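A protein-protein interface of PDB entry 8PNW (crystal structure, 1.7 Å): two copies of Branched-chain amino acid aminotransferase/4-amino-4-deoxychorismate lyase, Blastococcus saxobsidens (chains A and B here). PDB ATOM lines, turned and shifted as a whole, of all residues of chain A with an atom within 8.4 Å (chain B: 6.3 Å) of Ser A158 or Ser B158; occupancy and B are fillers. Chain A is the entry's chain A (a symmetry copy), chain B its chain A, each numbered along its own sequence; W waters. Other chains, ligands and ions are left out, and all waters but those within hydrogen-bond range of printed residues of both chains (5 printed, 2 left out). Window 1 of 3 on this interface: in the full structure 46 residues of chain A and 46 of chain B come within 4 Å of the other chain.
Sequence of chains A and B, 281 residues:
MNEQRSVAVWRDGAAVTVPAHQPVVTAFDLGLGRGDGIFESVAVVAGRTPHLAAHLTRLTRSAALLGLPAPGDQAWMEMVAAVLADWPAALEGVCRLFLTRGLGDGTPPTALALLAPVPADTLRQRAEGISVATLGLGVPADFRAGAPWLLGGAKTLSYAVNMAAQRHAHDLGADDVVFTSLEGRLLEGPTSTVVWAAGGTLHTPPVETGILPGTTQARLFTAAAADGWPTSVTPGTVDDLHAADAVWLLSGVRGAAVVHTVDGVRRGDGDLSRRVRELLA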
ATOM      1  N   LEU A  30     -22.487 -14.262 -37.670  1.00  0.00           N
ATOM      2  CA  LEU A  30     -21.453 -15.139 -37.086  1.00  0.00           C
ATOM      3  C   LEU A  30     -21.528 -15.125 -35.555  1.00  0.00           C
ATOM      4  O   LEU A  30     -20.969 -16.005 -34.949  1.00  0.00           O
ATOM      5  CB  LEU A  30     -20.117 -14.657 -37.620  1.00  0.00           C
ATOM      6  CG  LEU A  30     -19.814 -15.088 -39.049  1.00  0.00           C
ATOM      7  CD1 LEU A  30     -18.581 -14.355 -39.547  1.00  0.00           C
ATOM      8  CD2 LEU A  30     -19.621 -16.605 -39.128  1.00  0.00           C
ATOM      9  N   GLY A  31     -22.161 -14.128 -34.948  1.00  0.00           N
ATOM     10  CA  GLY A  31     -22.338 -14.094 -33.491  1.00  0.00           C
ATOM     11  C   GLY A  31     -23.251 -15.219 -33.043  1.00  0.00           C
ATOM     12  O   GLY A  31     -23.076 -15.711 -31.934  1.00  0.00           O
ATOM     13  N   LEU A  32     -24.241 -15.546 -33.872  1.00  0.00           N
ATOM     14  CA  LEU A  32     -25.169 -16.672 -33.632  1.00  0.00           C
ATOM     15  C   LEU A  32     -24.483 -17.975 -34.043  1.00  0.00           C
ATOM     16  O   LEU A  32     -24.486 -18.926 -33.239  1.00  0.00           O
ATOM     17  CB  LEU A  32     -26.438 -16.432 -34.456  1.00  0.00           C
ATOM     18  CG  LEU A  32     -27.461 -17.548 -34.408  1.00  0.00           C
ATOM     19  CD1 LEU A  32     -27.867 -17.835 -32.971  1.00  0.00           C
ATOM     20  CD2 LEU A  32     -28.653 -17.234 -35.300  1.00  0.00           C
ATOM     21  N   GLY A  33     -24.070 -18.041 -35.304  1.00  0.00           N
ATOM     22  CA  GLY A  33     -23.624 -19.314 -35.921  1.00  0.00           C
ATOM     23  C   GLY A  33     -22.332 -19.850 -35.349  1.00  0.00           C
ATOM     24  O   GLY A  33     -22.126 -21.072 -35.364  1.00  0.00           O
ATOM     25  N   ARG A  34     -21.433 -18.977 -34.919  1.00  0.00           N
ATOM     26  CA  ARG A  34     -20.100 -19.378 -34.416  1.00  0.00           C
ATOM     27  C   ARG A  34     -19.827 -18.796 -33.029  1.00  0.00           C
ATOM     28  O   ARG A  34     -18.792 -19.089 -32.489  1.00  0.00           O
ATOM     29  CB  ARG A  34     -19.028 -18.841 -35.373  1.00  0.00           C
ATOM     30  CG  ARG A  34     -19.059 -19.471 -36.766  1.00  0.00           C
ATOM     31  CD  ARG A  34     -18.796 -20.948 -36.703  1.00  0.00           C
ATOM     32  NE  ARG A  34     -18.516 -21.520 -38.032  1.00  0.00           N
ATOM     33  CZ  ARG A  34     -18.571 -22.833 -38.324  1.00  0.00           C
ATOM     34  NH1 ARG A  34     -18.952 -23.726 -37.421  1.00  0.00           N
ATOM     35  NH2 ARG A  34     -18.249 -23.252 -39.535  1.00  0.00           N
ATOM     36  N   GLY A  35     -20.723 -17.986 -32.463  1.00  0.00           N
ATOM     37  CA  GLY A  35     -20.424 -17.382 -31.149  1.00  0.00           C
ATOM     38  C   GLY A  35     -19.262 -16.438 -31.244  1.00  0.00           C
ATOM     39  O   GLY A  35     -18.535 -16.255 -30.251  1.00  0.00           O
ATOM     40  N   ASP A  36     -19.120 -15.834 -32.427  1.00  0.00           N
ATOM     41  CA  ASP A  36     -17.945 -15.063 -32.851  1.00  0.00           C
ATOM     42  C   ASP A  36     -18.236 -13.590 -32.587  1.00  0.00           C
ATOM     43  O   ASP A  36     -18.669 -12.860 -33.475  1.00  0.00           O
ATOM     44  CB  ASP A  36     -17.565 -15.377 -34.288  1.00  0.00           C
ATOM     45  CG  ASP A  36     -16.166 -14.904 -34.631  1.00  0.00           C
ATOM     46  OD1 ASP A  36     -15.438 -14.417 -33.700  1.00  0.00           O
ATOM     47  OD2 ASP A  36     -15.852 -14.947 -35.836  1.00  0.00           O
ATOM     48  N   GLY A  37     -18.040 -13.197 -31.345  1.00  0.00           N
ATOM     49  CA  GLY A  37     -18.316 -11.825 -30.914  1.00  0.00           C
ATOM     50  C   GLY A  37     -17.886 -11.639 -29.479  1.00  0.00           C
ATOM     51  O   GLY A  37     -17.431 -12.626 -28.796  1.00  0.00           O
ATOM     52  N   ILE A  38     -18.020 -10.407 -29.007  1.00  0.00           N
ATOM     53  CA  ILE A  38     -17.646 -10.069 -27.623  1.00  0.00           C
ATOM     54  C   ILE A  38     -18.826  -9.350 -26.979  1.00  0.00           C
ATOM     55  O   ILE A  38     -19.742  -8.932 -27.671  1.00  0.00           O
ATOM     56  CB  ILE A  38     -16.319  -9.282 -27.602  1.00  0.00           C
ATOM     57  CG1 ILE A  38     -16.382  -7.958 -28.353  1.00  0.00           C
ATOM     58  CG2 ILE A  38     -15.190 -10.138 -28.130  1.00  0.00           C
ATOM     59  CD1 ILE A  38     -16.972  -6.844 -27.568  1.00  0.00           C
ATOM     60  N   PHE A  39     -18.814  -9.254 -25.660  1.00  0.00           N
ATOM     61  CA  PHE A  39     -19.859  -8.517 -24.919  1.00  0.00           C
ATOM     62  C   PHE A  39     -19.281  -7.853 -23.669  1.00  0.00           C
ATOM     63  O   PHE A  39     -18.209  -8.184 -23.187  1.00  0.00           O
ATOM     64  CB  PHE A  39     -21.051  -9.415 -24.574  1.00  0.00           C
ATOM     65  CG  PHE A  39     -20.849 -10.294 -23.387  1.00  0.00           C
ATOM     66  CD1 PHE A  39     -20.038 -11.415 -23.474  1.00  0.00           C
ATOM     67  CD2 PHE A  39     -21.479 -10.030 -22.177  1.00  0.00           C
ATOM     68  CE1 PHE A  39     -19.834 -12.226 -22.375  1.00  0.00           C
ATOM     69  CE2 PHE A  39     -21.310 -10.870 -21.091  1.00  0.00           C
ATOM     70  CZ  PHE A  39     -20.475 -11.967 -21.183  1.00  0.00           C
ATOM     71  N   LEU A  66     -10.136 -10.488 -30.589  1.00  0.00           N
ATOM     72  CA  LEU A  66     -10.840 -11.303 -31.632  1.00  0.00           C
ATOM     73  C   LEU A  66     -10.686 -10.661 -33.020  1.00  0.00           C
ATOM     74  O   LEU A  66     -11.298 -11.117 -34.001  1.00  0.00           O
ATOM     75  CB  LEU A  66     -12.319 -11.505 -31.265  1.00  0.00           C
ATOM     76  CG  LEU A  66     -12.609 -12.668 -30.323  1.00  0.00           C
ATOM     77  CD1 LEU A  66     -12.161 -12.357 -28.896  1.00  0.00           C
ATOM     78  CD2 LEU A  66     -14.091 -13.037 -30.375  1.00  0.00           C
ATOM     79  N   LEU A 150      -6.939 -19.382 -27.822  1.00  0.00           N
ATOM     80  CA  LEU A 150      -7.916 -19.843 -26.778  1.00  0.00           C
ATOM     81  C   LEU A 150      -8.715 -18.665 -26.215  1.00  0.00           C
ATOM     82  O   LEU A 150      -9.624 -18.917 -25.434  1.00  0.00           O
ATOM     83  CB  LEU A 150      -7.214 -20.625 -25.670  1.00  0.00           C
ATOM     84  CG  LEU A 150      -6.501 -21.914 -26.103  1.00  0.00           C
ATOM     85  CD1 LEU A 150      -5.783 -22.592 -24.930  1.00  0.00           C
ATOM     86  CD2 LEU A 150      -7.441 -22.895 -26.768  1.00  0.00           C
ATOM     87  N   LEU A 151      -8.394 -17.441 -26.642  1.00  0.00           N
ATOM     88  CA  LEU A 151      -9.124 -16.185 -26.309  1.00  0.00           C
ATOM     89  C   LEU A 151      -9.207 -15.998 -24.788  1.00  0.00           C
ATOM     90  O   LEU A 151     -10.197 -15.428 -24.283  1.00  0.00           O
ATOM     91  CB  LEU A 151     -10.500 -16.201 -26.964  1.00  0.00           C
ATOM     92  CG  LEU A 151     -10.484 -16.365 -28.487  1.00  0.00           C
ATOM     93  CD1 LEU A 151     -11.904 -16.388 -29.025  1.00  0.00           C
ATOM     94  CD2 LEU A 151      -9.634 -15.286 -29.137  1.00  0.00           C
ATOM     95  N   ALA A 154     -10.574 -12.484 -23.026  1.00  0.00           N
ATOM     96  CA  ALA A 154     -11.631 -11.879 -23.866  1.00  0.00           C
ATOM     97  C   ALA A 154     -12.987 -12.296 -23.309  1.00  0.00           C
ATOM     98  O   ALA A 154     -13.125 -13.474 -22.924  1.00  0.00           O
ATOM     99  CB  ALA A 154     -11.489 -12.256 -25.337  1.00  0.00           C
ATOM    100  N   LYS A 155     -13.929 -11.348 -23.248  1.00  0.00           N
ATOM    101  CA  LYS A 155     -15.307 -11.564 -22.759  1.00  0.00           C
ATOM    102  C   LYS A 155     -16.135 -11.861 -24.005  1.00  0.00           C
ATOM    103  O   LYS A 155     -16.505 -10.924 -24.690  1.00  0.00           O
ATOM    104  CB  LYS A 155     -15.803 -10.359 -21.959  1.00  0.00           C
ATOM    105  CG  LYS A 155     -17.014 -10.595 -21.063  1.00  0.00           C
ATOM    106  CD  LYS A 155     -17.284  -9.409 -20.103  1.00  0.00           C
ATOM    107  CE  LYS A 155     -18.406  -9.600 -19.096  1.00  0.00           C
ATOM    108  NZ  LYS A 155     -18.205 -10.763 -18.237  1.00  0.00           N
ATOM    109  N   THR A 156     -16.369 -13.144 -24.318  1.00  0.00           N
ATOM    110  CA  THR A 156     -16.916 -13.524 -25.646  1.00  0.00           C
ATOM    111  C   THR A 156     -18.349 -14.033 -25.558  1.00  0.00           C
ATOM    112  O   THR A 156     -18.842 -14.378 -24.466  1.00  0.00           O
ATOM    113  CB  THR A 156     -16.054 -14.577 -26.342  1.00  0.00           C
ATOM    114  OG1 THR A 156     -16.341 -15.844 -25.754  1.00  0.00           O
ATOM    115  CG2 THR A 156     -14.579 -14.262 -26.227  1.00  0.00           C
ATOM    116  N   LEU A 157     -18.971 -14.144 -26.726  1.00  0.00           N
ATOM    117  CA  LEU A 157     -20.297 -14.755 -26.839  1.00  0.00           C
ATOM    118  C   LEU A 157     -20.203 -16.281 -26.808  1.00  0.00           C
ATOM    119  O   LEU A 157     -21.292 -16.898 -26.853  1.00  0.00           O
ATOM    120  CB  LEU A 157     -20.932 -14.277 -28.146  1.00  0.00           C
ATOM    121  CG  LEU A 157     -21.188 -12.773 -28.268  1.00  0.00           C
ATOM    122  CD1 LEU A 157     -21.846 -12.469 -29.590  1.00  0.00           C
ATOM    123  CD2 LEU A 157     -22.034 -12.268 -27.125  1.00  0.00           C
ATOM    124  N   SER A 158     -19.023 -16.882 -26.770  1.00  0.00           N
ATOM    125  CA  SER A 158     -18.874 -18.362 -26.867  1.00  0.00           C
ATOM    126  C   SER A 158     -18.830 -18.941 -25.452  1.00  0.00           C
ATOM    127  O   SER A 158     -17.775 -19.454 -25.027  1.00  0.00           O
ATOM    128  CB  SER A 158     -17.688 -18.772 -27.710  1.00  0.00           C
ATOM    129  OG  SER A 158     -18.022 -18.696 -29.086  1.00  0.00           O
ATOM    130  N   TYR A 159     -19.936 -18.838 -24.714  1.00  0.00           N
ATOM    131  CA  TYR A 159     -19.976 -19.193 -23.278  1.00  0.00           C
ATOM    132  C   TYR A 159     -20.820 -20.453 -23.047  1.00  0.00           C
ATOM    133  O   TYR A 159     -21.362 -20.687 -21.927  1.00  0.00           O
ATOM    134  CB  TYR A 159     -20.494 -18.003 -22.471  1.00  0.00           C
ATOM    135  CG  TYR A 159     -19.453 -17.069 -21.926  1.00  0.00           C
ATOM    136  CD1 TYR A 159     -18.195 -16.939 -22.509  1.00  0.00           C
ATOM    137  CD2 TYR A 159     -19.736 -16.341 -20.775  1.00  0.00           C
ATOM    138  CE1 TYR A 159     -17.259 -16.036 -22.005  1.00  0.00           C
ATOM    139  CE2 TYR A 159     -18.805 -15.452 -20.261  1.00  0.00           C
ATOM    140  CZ  TYR A 159     -17.597 -15.262 -20.912  1.00  0.00           C
ATOM    141  OH  TYR A 159     -16.684 -14.382 -20.398  1.00  0.00           O
ATOM    142  N   ALA A 160     -20.945 -21.331 -24.053  1.00  0.00           N
ATOM    143  CA  ALA A 160     -21.713 -22.570 -23.825  1.00  0.00           C
ATOM    144  C   ALA A 160     -21.107 -23.345 -22.653  1.00  0.00           C
ATOM    145  O   ALA A 160     -21.893 -23.919 -21.845  1.00  0.00           O
ATOM    146  CB  ALA A 160     -21.819 -23.420 -25.049  1.00  0.00           C
ATOM    147  N   VAL A 161     -19.795 -23.398 -22.560  1.00  0.00           N
ATOM    148  CA  VAL A 161     -19.123 -24.137 -21.465  1.00  0.00           C
ATOM    149  C   VAL A 161     -19.386 -23.442 -20.117  1.00  0.00           C
ATOM    150  O   VAL A 161     -19.716 -24.147 -19.140  1.00  0.00           O
ATOM    151  CB  VAL A 161     -17.624 -24.306 -21.752  1.00  0.00           C
ATOM    152  CG1 VAL A 161     -16.889 -24.765 -20.499  1.00  0.00           C
ATOM    153  CG2 VAL A 161     -17.422 -25.282 -22.907  1.00  0.00           C
ATOM    154  N   ASN A 162     -19.259 -22.130 -20.086  1.00  0.00           N
ATOM    155  CA  ASN A 162     -19.579 -21.283 -18.911  1.00  0.00           C
ATOM    156  C   ASN A 162     -20.964 -21.636 -18.379  1.00  0.00           C
ATOM    157  O   ASN A 162     -21.101 -21.941 -17.182  1.00  0.00           O
ATOM    158  CB  ASN A 162     -19.463 -19.827 -19.289  1.00  0.00           C
ATOM    159  CG  ASN A 162     -18.094 -19.515 -19.862  1.00  0.00           C
ATOM    160  OD1 ASN A 162     -17.717 -20.049 -20.934  1.00  0.00           O
ATOM    161  ND2 ASN A 162     -17.383 -18.609 -19.216  1.00  0.00           N
ATOM    162  N   MET A 163     -21.962 -21.706 -19.251  1.00  0.00           N
ATOM    163  CA  MET A 163     -23.349 -22.014 -18.842  1.00  0.00           C
ATOM    164  C   MET A 163     -23.508 -23.494 -18.483  1.00  0.00           C
ATOM    165  O   MET A 163     -24.227 -23.786 -17.525  1.00  0.00           O
ATOM    166  CB  MET A 163     -24.352 -21.642 -19.943  1.00  0.00           C
ATOM    167  CG  MET A 163     -24.295 -20.196 -20.369  1.00  0.00           C
ATOM    168  SD  MET A 163     -24.771 -19.047 -19.087  1.00  0.00           S
ATOM    169  CE  MET A 163     -23.200 -18.438 -18.490  1.00  0.00           C
ATOM    170  N   LEU B  32     -27.298 -16.420 -29.345  1.00  0.00           N
ATOM    171  CA  LEU B  32     -26.489 -15.221 -29.651  1.00  0.00           C
ATOM    172  C   LEU B  32     -25.681 -14.838 -28.409  1.00  0.00           C
ATOM    173  O   LEU B  32     -24.459 -14.639 -28.535  1.00  0.00           O
ATOM    174  CB  LEU B  32     -27.439 -14.092 -30.061  1.00  0.00           C
ATOM    175  CG  LEU B  32     -26.781 -12.751 -30.312  1.00  0.00           C
ATOM    176  CD1 LEU B  32     -25.700 -12.880 -31.374  1.00  0.00           C
ATOM    177  CD2 LEU B  32     -27.816 -11.691 -30.659  1.00  0.00           C
ATOM    178  N   GLY B  33     -26.388 -14.591 -27.312  1.00  0.00           N
ATOM    179  CA  GLY B  33     -25.783 -13.967 -26.110  1.00  0.00           C
ATOM    180  C   GLY B  33     -24.778 -14.847 -25.404  1.00  0.00           C
ATOM    181  O   GLY B  33     -23.857 -14.320 -24.764  1.00  0.00           O
ATOM    182  N   ARG B  34     -24.967 -16.158 -25.440  1.00  0.00           N
ATOM    183  CA  ARG B  34     -24.097 -17.115 -24.718  1.00  0.00           C
ATOM    184  C   ARG B  34     -23.559 -18.197 -25.654  1.00  0.00           C
ATOM    185  O   ARG B  34     -22.800 -19.011 -25.196  1.00  0.00           O
ATOM    186  CB  ARG B  34     -24.922 -17.804 -23.624  1.00  0.00           C
ATOM    187  CG  ARG B  34     -25.385 -16.869 -22.505  1.00  0.00           C
ATOM    188  CD  ARG B  34     -24.218 -16.274 -21.772  1.00  0.00           C
ATOM    189  NE  ARG B  34     -24.623 -15.625 -20.514  1.00  0.00           N
ATOM    190  CZ  ARG B  34     -23.867 -14.744 -19.831  1.00  0.00           C
ATOM    191  NH1 ARG B  34     -22.692 -14.342 -20.293  1.00  0.00           N
ATOM    192  NH2 ARG B  34     -24.300 -14.258 -18.682  1.00  0.00           N
ATOM    193  N   GLY B  35     -23.942 -18.218 -26.931  1.00  0.00           N
ATOM    194  CA  GLY B  35     -23.463 -19.302 -27.813  1.00  0.00           C
ATOM    195  C   GLY B  35     -24.001 -20.631 -27.370  1.00  0.00           C
ATOM    196  O   GLY B  35     -23.348 -21.665 -27.595  1.00  0.00           O
ATOM    197  N   ASP B  36     -25.196 -20.586 -26.772  1.00  0.00           N
ATOM    198  CA  ASP B  36     -25.821 -21.696 -26.043  1.00  0.00           C
ATOM    199  C   ASP B  36     -26.776 -22.401 -27.001  1.00  0.00           C
ATOM    200  O   ASP B  36     -27.973 -22.126 -27.019  1.00  0.00           O
ATOM    201  CB  ASP B  36     -26.468 -21.217 -24.755  1.00  0.00           C
ATOM    202  CG  ASP B  36     -26.782 -22.359 -23.808  1.00  0.00           C
ATOM    203  OD1 ASP B  36     -26.391 -23.537 -24.117  1.00  0.00           O
ATOM    204  OD2 ASP B  36     -27.486 -22.075 -22.821  1.00  0.00           O
ATOM    205  N   GLY B  37     -26.209 -23.264 -27.818  1.00  0.00           N
ATOM    206  CA  GLY B  37     -26.978 -23.992 -28.830  1.00  0.00           C
ATOM    207  C   GLY B  37     -26.090 -24.991 -29.531  1.00  0.00           C
ATOM    208  O   GLY B  37     -24.836 -25.057 -29.264  1.00  0.00           O
ATOM    209  N   THR B 156     -21.315 -27.366 -31.193  1.00  0.00           N
ATOM    210  CA  THR B 156     -22.012 -26.218 -30.557  1.00  0.00           C
ATOM    211  C   THR B 156     -21.846 -24.929 -31.350  1.00  0.00           C
ATOM    212  O   THR B 156     -20.966 -24.822 -32.227  1.00  0.00           O
ATOM    213  CB  THR B 156     -21.543 -25.986 -29.122  1.00  0.00           C
ATOM    214  OG1 THR B 156     -20.284 -25.318 -29.168  1.00  0.00           O
ATOM    215  CG2 THR B 156     -21.427 -27.282 -28.351  1.00  0.00           C
ATOM    216  N   LEU B 157     -22.648 -23.939 -30.974  1.00  0.00           N
ATOM    217  CA  LEU B 157     -22.520 -22.589 -31.527  1.00  0.00           C
ATOM    218  C   LEU B 157     -21.369 -21.831 -30.866  1.00  0.00           C
ATOM    219  O   LEU B 157     -21.148 -20.679 -31.304  1.00  0.00           O
ATOM    220  CB  LEU B 157     -23.847 -21.858 -31.311  1.00  0.00           C
ATOM    221  CG  LEU B 157     -25.072 -22.448 -32.013  1.00  0.00           C
ATOM    222  CD1 LEU B 157     -26.285 -21.599 -31.732  1.00  0.00           C
ATOM    223  CD2 LEU B 157     -24.843 -22.573 -33.499  1.00  0.00           C
ATOM    224  N   SER B 158     -20.688 -22.377 -29.869  1.00  0.00           N
ATOM    225  CA  SER B 158     -19.644 -21.633 -29.108  1.00  0.00           C
ATOM    226  C   SER B 158     -18.282 -21.921 -29.742  1.00  0.00           C
ATOM    227  O   SER B 158     -17.434 -22.581 -29.108  1.00  0.00           O
ATOM    228  CB  SER B 158     -19.682 -21.931 -27.627  1.00  0.00           C
ATOM    229  OG  SER B 158     -20.705 -21.170 -27.006  1.00  0.00           O
ATOM    230  N   TYR B 159     -18.074 -21.470 -30.979  1.00  0.00           N
ATOM    231  CA  TYR B 159     -16.878 -21.828 -31.772  1.00  0.00           C
ATOM    232  C   TYR B 159     -15.961 -20.613 -31.962  1.00  0.00           C
ATOM    233  O   TYR B 159     -15.152 -20.544 -32.934  1.00  0.00           O
ATOM    234  CB  TYR B 159     -17.310 -22.432 -33.107  1.00  0.00           C
ATOM    235  CG  TYR B 159     -17.442 -23.928 -33.147  1.00  0.00           C
ATOM    236  CD1 TYR B 159     -17.689 -24.680 -32.002  1.00  0.00           C
ATOM    237  CD2 TYR B 159     -17.267 -24.588 -34.358  1.00  0.00           C
ATOM    238  CE1 TYR B 159     -17.845 -26.065 -32.071  1.00  0.00           C
ATOM    239  CE2 TYR B 159     -17.408 -25.965 -34.432  1.00  0.00           C
ATOM    240  CZ  TYR B 159     -17.752 -26.686 -33.301  1.00  0.00           C
ATOM    241  OH  TYR B 159     -17.888 -28.046 -33.383  1.00  0.00           O
ATOM    242  N   ALA B 160     -16.005 -19.631 -31.050  1.00  0.00           N
ATOM    243  CA  ALA B 160     -15.092 -18.482 -31.198  1.00  0.00           C
ATOM    244  C   ALA B 160     -13.644 -18.973 -31.227  1.00  0.00           C
ATOM    245  O   ALA B 160     -12.837 -18.413 -32.023  1.00  0.00           O
ATOM    246  CB  ALA B 160     -15.297 -17.440 -30.147  1.00  0.00           C
ATOM    247  N   VAL B 161     -13.302 -19.940 -30.401  1.00  0.00           N
ATOM    248  CA  VAL B 161     -11.919 -20.469 -30.352  1.00  0.00           C
ATOM    249  C   VAL B 161     -11.586 -21.206 -31.662  1.00  0.00           C
ATOM    250  O   VAL B 161     -10.490 -20.974 -32.212  1.00  0.00           O
ATOM    251  CB  VAL B 161     -11.709 -21.353 -29.115  1.00  0.00           C
ATOM    252  CG1 VAL B 161     -10.413 -22.146 -29.239  1.00  0.00           C
ATOM    253  CG2 VAL B 161     -11.719 -20.495 -27.854  1.00  0.00           C
ATOM    254  N   ASN B 162     -12.501 -22.033 -32.131  1.00  0.00           N
ATOM    255  CA  ASN B 162     -12.404 -22.742 -33.430  1.00  0.00           C
ATOM    256  C   ASN B 162     -12.051 -21.752 -34.536  1.00  0.00           C
ATOM    257  O   ASN B 162     -11.065 -21.971 -35.261  1.00  0.00           O
ATOM    258  CB  ASN B 162     -13.694 -23.474 -33.705  1.00  0.00           C
ATOM    259  CG  ASN B 162     -14.047 -24.412 -32.567  1.00  0.00           C
ATOM    260  OD1 ASN B 162     -14.295 -23.958 -31.423  1.00  0.00           O
ATOM    261  ND2 ASN B 162     -14.154 -25.691 -32.877  1.00  0.00           N
HETATM  262  O   HOH W   1     -20.259 -23.136 -34.702  1.00  0.00           O
HETATM  263  O   HOH W   2     -24.538 -24.591 -22.556  1.00  0.00           O
HETATM  264  O   HOH W   3     -13.300 -15.823 -33.041  1.00  0.00           O
HETATM  265  O   HOH W   4     -27.717 -20.543 -20.769  1.00  0.00           O
HETATM  266  O   HOH W   5     -21.572 -14.816 -23.116  1.00  0.00           O
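Arg A34 touches Ala B160, and with the chains exchanged Ala A160 touches Arg B34. Gly A35 touches Leu B157, and with the chains exchanged Leu A157 touches Gly B35. Gly A35 touches Ala B160, and with the chains exchanged Ala A160 touches Gly B35. Ser A158 touches Tyr B159, and with the chains exchanged Tyr A159 touches Ser B158. Positions printed for both chains: 32, 33, 34, 35, 36, 37, 156, 157, 158, 159, 160, 161 and 162. Of the 27 pairs that touch across the chains among the printed residues, 22 have their exchanged pair printed and touching as well.
O of Arg B34 sits at hydrogen-bond distance from N of Tyr A159 (2.9 Å). The backbone NH (N) of Ala A160 is in hydrogen-bond range of the backbone carbonyl oxygen (O) of Arg B34, at 3.2 Å. The side-chain sulfur (SD) of Met A163 sits at hydrogen-bond distance from the guanidinium group (NE) of Arg B34. The backbone carbonyl oxygen of Leu A157 lies within hydrogen-bond range of the backbone NH of Gly B35, 3.0 Å away. The backbone carbonyl oxygen of Leu B157 is in hydrogen-bond range of the backbone NH of Gly A35 (3.0 Å). OG of Ser B158 is in hydrogen-bond range of N of Tyr A159 (3.4 Å). The backbone NH (N) of Ala A160 is in hydrogen-bond range of the side-chain hydroxyl (OG) of Ser B158 (3.0 Å). N of Tyr B159 sits at hydrogen-bond distance from O of Arg A34, at 2.9 Å. The backbone NH (N) of Tyr B159 is in hydrogen-bond range of the side-chain hydroxyl (OG) of Ser A158 (3.4 Å). The backbone NH (N) of Ala B160 sits at hydrogen-bond distance from the backbone carbonyl oxygen (O) of Arg A34, at 3.2 Å. The side-chain hydroxyl (OG) of Ser A158 lies within hydrogen-bond range of the backbone NH (N) of Ala B160, at 3.0 Å. The backbone carbonyl oxygen (O) of Leu B157 lies close to the backbone carbonyl oxygen (O) of Arg A34. The backbone carbonyl oxygen (O) of Leu A157 lies close to the backbone carbonyl oxygen (O) of Arg B34, 3.1 Å away.
Printed residues of chain B within 4 Å of Gly A31: Leu B32. Of chain B, only Arg B34, Ser B158, Tyr B159 and Ala B160 come within 4 Å of Ser A158. Of the printed residues of chain B, Ala A160 touches Arg B34, Gly B35 and Ser B158. Of the printed residues of chain A, Arg B34 touches Phe A39, Leu A157, Ser A158, Tyr A159, Ala A160 and Met A163. Of the printed residues of chain A, Gly B35 touches Leu A157 (3.0 Å) and Ala A160 (3.4 Å). Ser B158 touches just these residues of chain A: Arg A34 (3.98 Å), Ser A158 (3.3 Å), Tyr A159 (3.4 Å) and Ala A160 (3.0 Å). The nearest residue of chain B that does not touch Ser A158 is Leu B157 (4.3 Å). The nearest residue of chain A that does not touch Ser B158 is Leu A157 (4.3 Å).
Of the 23 printed residues of chain A, 13 touch a printed residue of chain B. Hydrophobic or aromatic side chains of chain A within 4 Å of the printed part of chain B: Leu A32, Phe A39, Leu A150, Leu A151, Leu A157, Tyr A159, Ala A160 and Met A163. Among the printed residues, 27 pairs touch across the chains. Among the printed residues, no Asp or Glu carboxylate lies within 4 Å of a Lys or Arg side-chain nitrogen of the other chain.
Among the printed residues, merely in contact across the chains: Gly A31 with Leu B32, Leu A32 with Leu B32, Leu A32 with Leu B157, Gly A33 with Leu B157, Arg A34 with Ser B158, Gly A35 with Ala B160, Phe A39 with Arg B34, Leu A150 with Val B161, Leu A151 with Ala B160, Leu A157 with Leu B32, Leu A157 with Gly B33, Ser A158 with Arg B34, Ser A158 with Ser B158 and Ala A160 with Gly B35.
The side-chain hydroxyl (OG) of Ser B158 lies within hydrogen-bond range of the backbone carbonyl oxygen (O) of Gly B35. N of Leu B157 sits at hydrogen-bond distance from O of Gly B37, at 3.0 Å. N of Gly A35 sits at hydrogen-bond distance from O of Leu A30, at 3.2 Å. O of Gly A35 lies within hydrogen-bond range of OG of Ser A158 (2.8 Å). The backbone carbonyl oxygen (O) of Gly A37 is in hydrogen-bond range of the backbone NH (N) of Leu A157 (3.0 Å). The backbone NH (N) of Phe A39 lies within hydrogen-bond range of the backbone carbonyl oxygen (O) of Lys A155 (3.0 Å).
Water W4 lies within hydrogen-bond range of the side-chain carboxylate (OD2) of Asp B36 (2.6 Å) and the side-chain sulfur (SD) of Met A163 (3.7 Å). Water W2 bridges OD1 of Asp B36 (2.6 Å) and O of Ala A160 (2.8 Å). Water W3 bridges OD1 of Asp A36 (2.6 Å) and O of Ala B160 (2.8 Å). Water W1 lies within hydrogen-bond range of O of Gly A33, NH1 of Arg A34 and O of Thr B156. Water W5 lies within hydrogen-bond range of O of Gly B33 (2.9 Å), NH1 of Arg B34 (3.1 Å) and O of Thr A156 (3.1 Å).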
